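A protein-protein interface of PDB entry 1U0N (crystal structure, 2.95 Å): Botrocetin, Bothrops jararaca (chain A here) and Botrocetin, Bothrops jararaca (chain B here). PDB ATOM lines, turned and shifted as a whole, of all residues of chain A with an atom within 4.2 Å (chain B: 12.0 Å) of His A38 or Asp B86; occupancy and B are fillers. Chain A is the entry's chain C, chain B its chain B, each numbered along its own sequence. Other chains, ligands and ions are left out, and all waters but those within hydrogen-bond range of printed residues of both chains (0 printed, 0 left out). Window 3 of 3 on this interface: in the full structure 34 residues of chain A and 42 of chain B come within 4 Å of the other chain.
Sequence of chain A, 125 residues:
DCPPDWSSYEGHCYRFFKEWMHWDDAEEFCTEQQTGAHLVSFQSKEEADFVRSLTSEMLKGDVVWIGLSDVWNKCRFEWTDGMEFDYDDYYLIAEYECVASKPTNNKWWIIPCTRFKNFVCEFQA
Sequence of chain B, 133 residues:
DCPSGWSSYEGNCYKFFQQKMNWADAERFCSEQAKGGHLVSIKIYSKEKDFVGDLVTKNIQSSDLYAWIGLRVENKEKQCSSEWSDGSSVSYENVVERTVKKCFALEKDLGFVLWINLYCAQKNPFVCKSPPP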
ATOM      1  N   GLU A  27      25.519  17.389  33.873  1.00  0.00           N
ATOM      2  CA  GLU A  27      26.632  17.713  32.988  1.00  0.00           C
ATOM      3  C   GLU A  27      27.800  18.179  33.845  1.00  0.00           C
ATOM      4  O   GLU A  27      28.876  17.584  33.815  1.00  0.00           O
ATOM      5  CB  GLU A  27      26.239  18.825  32.011  1.00  0.00           C
ATOM      6  CG  GLU A  27      27.384  19.313  31.122  1.00  0.00           C
ATOM      7  CD  GLU A  27      27.710  18.366  29.977  1.00  0.00           C
ATOM      8  OE1 GLU A  27      27.285  17.189  30.025  1.00  0.00           O
ATOM      9  OE2 GLU A  27      28.404  18.800  29.031  1.00  0.00           O
ATOM     10  N   CYS A  30      29.441  15.277  35.619  1.00  0.00           N
ATOM     11  CA  CYS A  30      30.145  14.493  34.609  1.00  0.00           C
ATOM     12  C   CYS A  30      31.479  15.092  34.191  1.00  0.00           C
ATOM     13  O   CYS A  30      32.461  14.372  34.032  1.00  0.00           O
ATOM     14  CB  CYS A  30      29.293  14.332  33.358  1.00  0.00           C
ATOM     15  SG  CYS A  30      28.133  12.937  33.387  1.00  0.00           S
ATOM     16  N   THR A  31      31.517  16.404  33.999  1.00  0.00           N
ATOM     17  CA  THR A  31      32.754  17.043  33.583  1.00  0.00           C
ATOM     18  C   THR A  31      33.784  16.963  34.689  1.00  0.00           C
ATOM     19  O   THR A  31      34.897  16.496  34.466  1.00  0.00           O
ATOM     20  CB  THR A  31      32.538  18.523  33.201  1.00  0.00           C
ATOM     21  OG1 THR A  31      32.113  19.268  34.350  1.00  0.00           O
ATOM     22  CG2 THR A  31      31.485  18.635  32.105  1.00  0.00           C
ATOM     23  N   ALA A  37      35.039  15.024  29.910  1.00  0.00           N
ATOM     24  CA  ALA A  37      33.828  14.220  29.941  1.00  0.00           C
ATOM     25  C   ALA A  37      32.569  15.056  30.072  1.00  0.00           C
ATOM     26  O   ALA A  37      32.599  16.165  30.602  1.00  0.00           O
ATOM     27  CB  ALA A  37      33.901  13.228  31.080  1.00  0.00           C
ATOM     28  N   HIS A  38      31.464  14.505  29.577  1.00  0.00           N
ATOM     29  CA  HIS A  38      30.154  15.149  29.629  1.00  0.00           C
ATOM     30  C   HIS A  38      29.122  14.039  29.851  1.00  0.00           C
ATOM     31  O   HIS A  38      29.465  12.964  30.342  1.00  0.00           O
ATOM     32  CB  HIS A  38      29.873  15.885  28.313  1.00  0.00           C
ATOM     33  CG  HIS A  38      30.939  16.868  27.932  1.00  0.00           C
ATOM     34  ND1 HIS A  38      31.316  17.911  28.750  1.00  0.00           N
ATOM     35  CD2 HIS A  38      31.726  16.951  26.833  1.00  0.00           C
ATOM     36  CE1 HIS A  38      32.292  18.591  28.173  1.00  0.00           C
ATOM     37  NE2 HIS A  38      32.560  18.029  27.008  1.00  0.00           N
ATOM     38  N   LEU A  39      27.862  14.292  29.514  1.00  0.00           N
ATOM     39  CA  LEU A  39      26.832  13.267  29.671  1.00  0.00           C
ATOM     40  C   LEU A  39      26.895  12.278  28.505  1.00  0.00           C
ATOM     41  O   LEU A  39      27.269  12.644  27.390  1.00  0.00           O
ATOM     42  CB  LEU A  39      25.441  13.909  29.739  1.00  0.00           C
ATOM     43  CG  LEU A  39      24.963  14.384  31.115  1.00  0.00           C
ATOM     44  CD1 LEU A  39      23.654  15.139  30.972  1.00  0.00           C
ATOM     45  CD2 LEU A  39      24.782  13.181  32.035  1.00  0.00           C
ATOM     46  N   VAL A  40      26.538  11.024  28.762  1.00  0.00           N
ATOM     47  CA  VAL A  40      26.572  10.004  27.717  1.00  0.00           C
ATOM     48  C   VAL A  40      25.950  10.501  26.408  1.00  0.00           C
ATOM     49  O   VAL A  40      24.864  11.085  26.411  1.00  0.00           O
ATOM     50  CB  VAL A  40      25.835   8.706  28.166  1.00  0.00           C
ATOM     51  CG1 VAL A  40      24.381   8.997  28.488  1.00  0.00           C
ATOM     52  CG2 VAL A  40      25.921   7.666  27.071  1.00  0.00           C
ATOM     53  N   SER A  41      26.646  10.269  25.296  1.00  0.00           N
ATOM     54  CA  SER A  41      26.158  10.694  23.985  1.00  0.00           C
ATOM     55  C   SER A  41      26.002   9.538  22.991  1.00  0.00           C
ATOM     56  O   SER A  41      26.887   9.287  22.180  1.00  0.00           O
ATOM     57  CB  SER A  41      27.092  11.752  23.389  1.00  0.00           C
ATOM     58  OG  SER A  41      28.336  11.193  23.017  1.00  0.00           O
ATOM     59  N   CYS A 121      28.218   9.090  32.596  1.00  0.00           N
ATOM     60  CA  CYS A 121      29.272   9.937  32.038  1.00  0.00           C
ATOM     61  C   CYS A 121      30.240   9.154  31.150  1.00  0.00           C
ATOM     62  O   CYS A 121      30.593   8.021  31.466  1.00  0.00           O
ATOM     63  CB  CYS A 121      30.075  10.599  33.156  1.00  0.00           C
ATOM     64  SG  CYS A 121      29.106  11.485  34.420  1.00  0.00           S
ATOM     65  N   GLU A 122      30.665   9.760  30.042  1.00  0.00           N
ATOM     66  CA  GLU A 122      31.617   9.112  29.137  1.00  0.00           C
ATOM     67  C   GLU A 122      32.711  10.097  28.734  1.00  0.00           C
ATOM     68  O   GLU A 122      32.552  11.305  28.892  1.00  0.00           O
ATOM     69  CB  GLU A 122      30.925   8.572  27.865  1.00  0.00           C
ATOM     70  CG  GLU A 122      30.552   9.631  26.813  1.00  0.00           C
ATOM     71  CD  GLU A 122      30.600   9.103  25.368  1.00  0.00           C
ATOM     72  OE1 GLU A 122      31.703   8.755  24.886  1.00  0.00           O
ATOM     73  OE2 GLU A 122      29.538   9.042  24.709  1.00  0.00           O
ATOM     74  N   GLN B  79      13.964  16.909  17.665  1.00  0.00           N
ATOM     75  CA  GLN B  79      14.441  17.820  18.703  1.00  0.00           C
ATOM     76  C   GLN B  79      15.467  18.740  18.055  1.00  0.00           C
ATOM     77  O   GLN B  79      16.053  18.375  17.050  1.00  0.00           O
ATOM     78  CB  GLN B  79      15.043  17.029  19.870  1.00  0.00           C
ATOM     79  CG  GLN B  79      16.219  16.136  19.530  1.00  0.00           C
ATOM     80  CD  GLN B  79      17.535  16.877  19.570  1.00  0.00           C
ATOM     81  OE1 GLN B  79      17.770  17.684  20.465  1.00  0.00           O
ATOM     82  NE2 GLN B  79      18.409  16.597  18.611  1.00  0.00           N
ATOM     83  N   SER B  81      18.612  19.838  18.908  1.00  0.00           N
ATOM     84  CA  SER B  81      19.963  19.906  19.424  1.00  0.00           C
ATOM     85  C   SER B  81      20.792  19.098  18.431  1.00  0.00           C
ATOM     86  O   SER B  81      20.782  17.864  18.450  1.00  0.00           O
ATOM     87  CB  SER B  81      20.048  19.314  20.827  1.00  0.00           C
ATOM     88  OG  SER B  81      21.309  19.592  21.402  1.00  0.00           O
ATOM     89  N   SER B  82      21.487  19.812  17.547  1.00  0.00           N
ATOM     90  CA  SER B  82      22.306  19.190  16.512  1.00  0.00           C
ATOM     91  C   SER B  82      23.516  18.450  17.054  1.00  0.00           C
ATOM     92  O   SER B  82      23.954  17.468  16.465  1.00  0.00           O
ATOM     93  CB  SER B  82      22.752  20.245  15.504  1.00  0.00           C
ATOM     94  OG  SER B  82      23.255  21.383  16.175  1.00  0.00           O
ATOM     95  N   GLU B  83      24.063  18.921  18.165  1.00  0.00           N
ATOM     96  CA  GLU B  83      25.210  18.252  18.758  1.00  0.00           C
ATOM     97  C   GLU B  83      24.940  17.852  20.202  1.00  0.00           C
ATOM     98  O   GLU B  83      24.025  18.373  20.846  1.00  0.00           O
ATOM     99  CB  GLU B  83      26.449  19.147  18.710  1.00  0.00           C
ATOM    100  CG  GLU B  83      26.175  20.608  18.400  1.00  0.00           C
ATOM    101  CD  GLU B  83      25.849  20.834  16.935  1.00  0.00           C
ATOM    102  OE1 GLU B  83      25.794  22.009  16.512  1.00  0.00           O
ATOM    103  OE2 GLU B  83      25.648  19.838  16.203  1.00  0.00           O
ATOM    104  N   TRP B  84      25.728  16.904  20.699  1.00  0.00           N
ATOM    105  CA  TRP B  84      25.591  16.464  22.076  1.00  0.00           C
ATOM    106  C   TRP B  84      26.415  17.430  22.926  1.00  0.00           C
ATOM    107  O   TRP B  84      27.125  18.289  22.406  1.00  0.00           O
ATOM    108  CB  TRP B  84      26.124  15.037  22.278  1.00  0.00           C
ATOM    109  CG  TRP B  84      25.399  13.920  21.544  1.00  0.00           C
ATOM    110  CD1 TRP B  84      25.638  13.480  20.274  1.00  0.00           C
ATOM    111  CD2 TRP B  84      24.380  13.064  22.072  1.00  0.00           C
ATOM    112  NE1 TRP B  84      24.840  12.401  19.981  1.00  0.00           N
ATOM    113  CE2 TRP B  84      24.057  12.125  21.066  1.00  0.00           C
ATOM    114  CE3 TRP B  84      23.709  12.999  23.297  1.00  0.00           C
ATOM    115  CZ2 TRP B  84      23.092  11.132  21.246  1.00  0.00           C
ATOM    116  CZ3 TRP B  84      22.746  12.008  23.479  1.00  0.00           C
ATOM    117  CH2 TRP B  84      22.448  11.087  22.454  1.00  0.00           C
ATOM    118  N   SER B  85      26.313  17.283  24.238  1.00  0.00           N
ATOM    119  CA  SER B  85      27.047  18.133  25.158  1.00  0.00           C
ATOM    120  C   SER B  85      28.540  17.871  25.020  1.00  0.00           C
ATOM    121  O   SER B  85      29.351  18.473  25.720  1.00  0.00           O
ATOM    122  CB  SER B  85      26.615  17.824  26.587  1.00  0.00           C
ATOM    123  OG  SER B  85      26.813  16.448  26.868  1.00  0.00           O
ATOM    124  N   ASP B  86      28.897  16.964  24.120  1.00  0.00           N
ATOM    125  CA  ASP B  86      30.291  16.613  23.915  1.00  0.00           C
ATOM    126  C   ASP B  86      30.765  17.051  22.539  1.00  0.00           C
ATOM    127  O   ASP B  86      31.891  16.755  22.140  1.00  0.00           O
ATOM    128  CB  ASP B  86      30.463  15.109  24.039  1.00  0.00           C
ATOM    129  CG  ASP B  86      29.956  14.380  22.823  1.00  0.00           C
ATOM    130  OD1 ASP B  86      29.306  15.035  21.975  1.00  0.00           O
ATOM    131  OD2 ASP B  86      30.203  13.162  22.713  1.00  0.00           O
ATOM    132  N   GLY B  87      29.889  17.729  21.805  1.00  0.00           N
ATOM    133  CA  GLY B  87      30.243  18.207  20.478  1.00  0.00           C
ATOM    134  C   GLY B  87      29.929  17.229  19.369  1.00  0.00           C
ATOM    135  O   GLY B  87      29.689  17.632  18.229  1.00  0.00           O
ATOM    136  N   SER B  88      29.933  15.941  19.703  1.00  0.00           N
ATOM    137  CA  SER B  88      29.655  14.912  18.716  1.00  0.00           C
ATOM    138  C   SER B  88      28.293  15.176  18.092  1.00  0.00           C
ATOM    139  O   SER B  88      27.286  15.256  18.791  1.00  0.00           O
ATOM    140  CB  SER B  88      29.691  13.521  19.359  1.00  0.00           C
ATOM    141  OG  SER B  88      28.653  13.349  20.301  1.00  0.00           O
ATOM    142  N   SER B  89      28.268  15.321  16.771  1.00  0.00           N
ATOM    143  CA  SER B  89      27.028  15.596  16.057  1.00  0.00           C
ATOM    144  C   SER B  89      25.990  14.481  16.154  1.00  0.00           C
ATOM    145  O   SER B  89      26.306  13.305  15.994  1.00  0.00           O
ATOM    146  CB  SER B  89      27.332  15.888  14.589  1.00  0.00           C
ATOM    147  OG  SER B  89      28.154  17.038  14.476  1.00  0.00           O
ATOM    148  N   VAL B  90      24.748  14.875  16.416  1.00  0.00           N
ATOM    149  CA  VAL B  90      23.636  13.938  16.536  1.00  0.00           C
ATOM    150  C   VAL B  90      23.235  13.352  15.189  1.00  0.00           C
ATOM    151  O   VAL B  90      22.891  14.078  14.258  1.00  0.00           O
ATOM    152  CB  VAL B  90      22.399  14.621  17.171  1.00  0.00           C
ATOM    153  CG1 VAL B  90      21.130  13.810  16.881  1.00  0.00           C
ATOM    154  CG2 VAL B  90      22.611  14.756  18.677  1.00  0.00           C
ATOM    155  N   SER B  91      23.279  12.026  15.112  1.00  0.00           N
ATOM    156  CA  SER B  91      22.924  11.287  13.906  1.00  0.00           C
ATOM    157  C   SER B  91      21.839  10.267  14.253  1.00  0.00           C
ATOM    158  O   SER B  91      20.702  10.370  13.795  1.00  0.00           O
ATOM    159  CB  SER B  91      24.157  10.566  13.368  1.00  0.00           C
ATOM    160  OG  SER B  91      24.758   9.786  14.392  1.00  0.00           O
ATOM    161  N   TYR B  92      22.202   9.281  15.066  1.00  0.00           N
ATOM    162  CA  TYR B  92      21.271   8.247  15.500  1.00  0.00           C
ATOM    163  C   TYR B  92      20.490   8.714  16.714  1.00  0.00           C
ATOM    164  O   TYR B  92      21.022   8.729  17.827  1.00  0.00           O
ATOM    165  CB  TYR B  92      22.025   6.982  15.884  1.00  0.00           C
ATOM    166  CG  TYR B  92      21.251   6.053  16.797  1.00  0.00           C
ATOM    167  CD1 TYR B  92      20.150   5.341  16.329  1.00  0.00           C
ATOM    168  CD2 TYR B  92      21.653   5.849  18.117  1.00  0.00           C
ATOM    169  CE1 TYR B  92      19.472   4.431  17.150  1.00  0.00           C
ATOM    170  CE2 TYR B  92      20.982   4.943  18.949  1.00  0.00           C
ATOM    171  CZ  TYR B  92      19.894   4.232  18.459  1.00  0.00           C
ATOM    172  OH  TYR B  92      19.244   3.308  19.256  1.00  0.00           O
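The side-chain hydroxyl of Ser B85 sits at hydrogen-bond distance from the side-chain carboxylate of Glu A27 (3.3 Å). The backbone carbonyl oxygen of Ser B85 lies close to a ring nitrogen (NE2) of His A38 (3.5 Å). The side-chain carboxylate (OD2) of Asp B86 lies within hydrogen-bond range of the side-chain hydroxyl (OG) of Ser A41 (2.7 Å). The side-chain hydroxyl (OG) of Ser B88 lies within hydrogen-bond range of the side-chain hydroxyl (OG) of Ser A41 (3.5 Å).
Of chain B, only Ser B85 comes within 4 Å of Glu A27. No residue of chain B comes within 4 Å of Cys A30. No residue of chain B comes within 4 Å of Thr A31. Of the printed residues of chain B, Leu A39 touches Ser B85 (3.6 Å). Val A40 touches just one residue of chain B: Trp B84. No residue of chain B comes within 4 Å of Glu A122. Of the printed residues of chain A, Trp B84 touches Val A40 and Ser A41. Printed residues of chain A within 4 Å of Ser B85: Glu A27 (3.2 Å), His A38 (3.0 Å) and Leu A39 (3.6 Å). Asp B86 touches two residues of chain A. Of the printed residues of chain A, Ser B88 touches Ser A41. Ser B89 touches none of the printed residues of chain A. Tyr B92 touches none of the printed residues of chain A. The nearest printed residue of chain A that does not touch Asp B86 is Glu A122 (4.6 Å). The nearest printed residue of chain A that does not touch Ser B88 is Glu A122 (6.2 Å).
The side-chain hydroxyl (OG) of Ser B88 is in hydrogen-bond range of the side-chain carboxylate (OD1) of Asp B86 (2.5 Å). ND1 of His A38 lies within hydrogen-bond range of OE2 of Glu A27 (3.1 Å). The side-chain carboxylate (OE1) of Glu A27 is in hydrogen-bond range of the backbone NH (N) of Leu A39, at 3.0 Å. The backbone carbonyl oxygen of His A38 lies within hydrogen-bond range of the backbone NH of Glu A122 (3.4 Å). The side-chain carboxylate of Glu A122 sits at hydrogen-bond distance from the side-chain hydroxyl of Ser A41. The side-chain sulfur (SG) of Cys A121 forms a disulfide with the side-chain sulfur (SG) of Cys A30 (2.0 Å).
Among the printed residues, pairs that only touch across the chains: His A38 with Asp B86, Ser A41 with Trp B84, Leu A39 with Ser B85 and Val A40 with Trp B84.
Hydrophobic or aromatic side chains of chain A within 4 Å of the printed part of chain B: His A38. Along chain A the printed residues that touch a printed residue of chain B span positions 27 to 41. Of the 13 printed residues of chain B, 4 touch a printed residue of chain A. Among the printed residues, no Asp or Glu carboxylate lies within 4 Å of a Lys or Arg side-chain nitrogen of the other chain.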
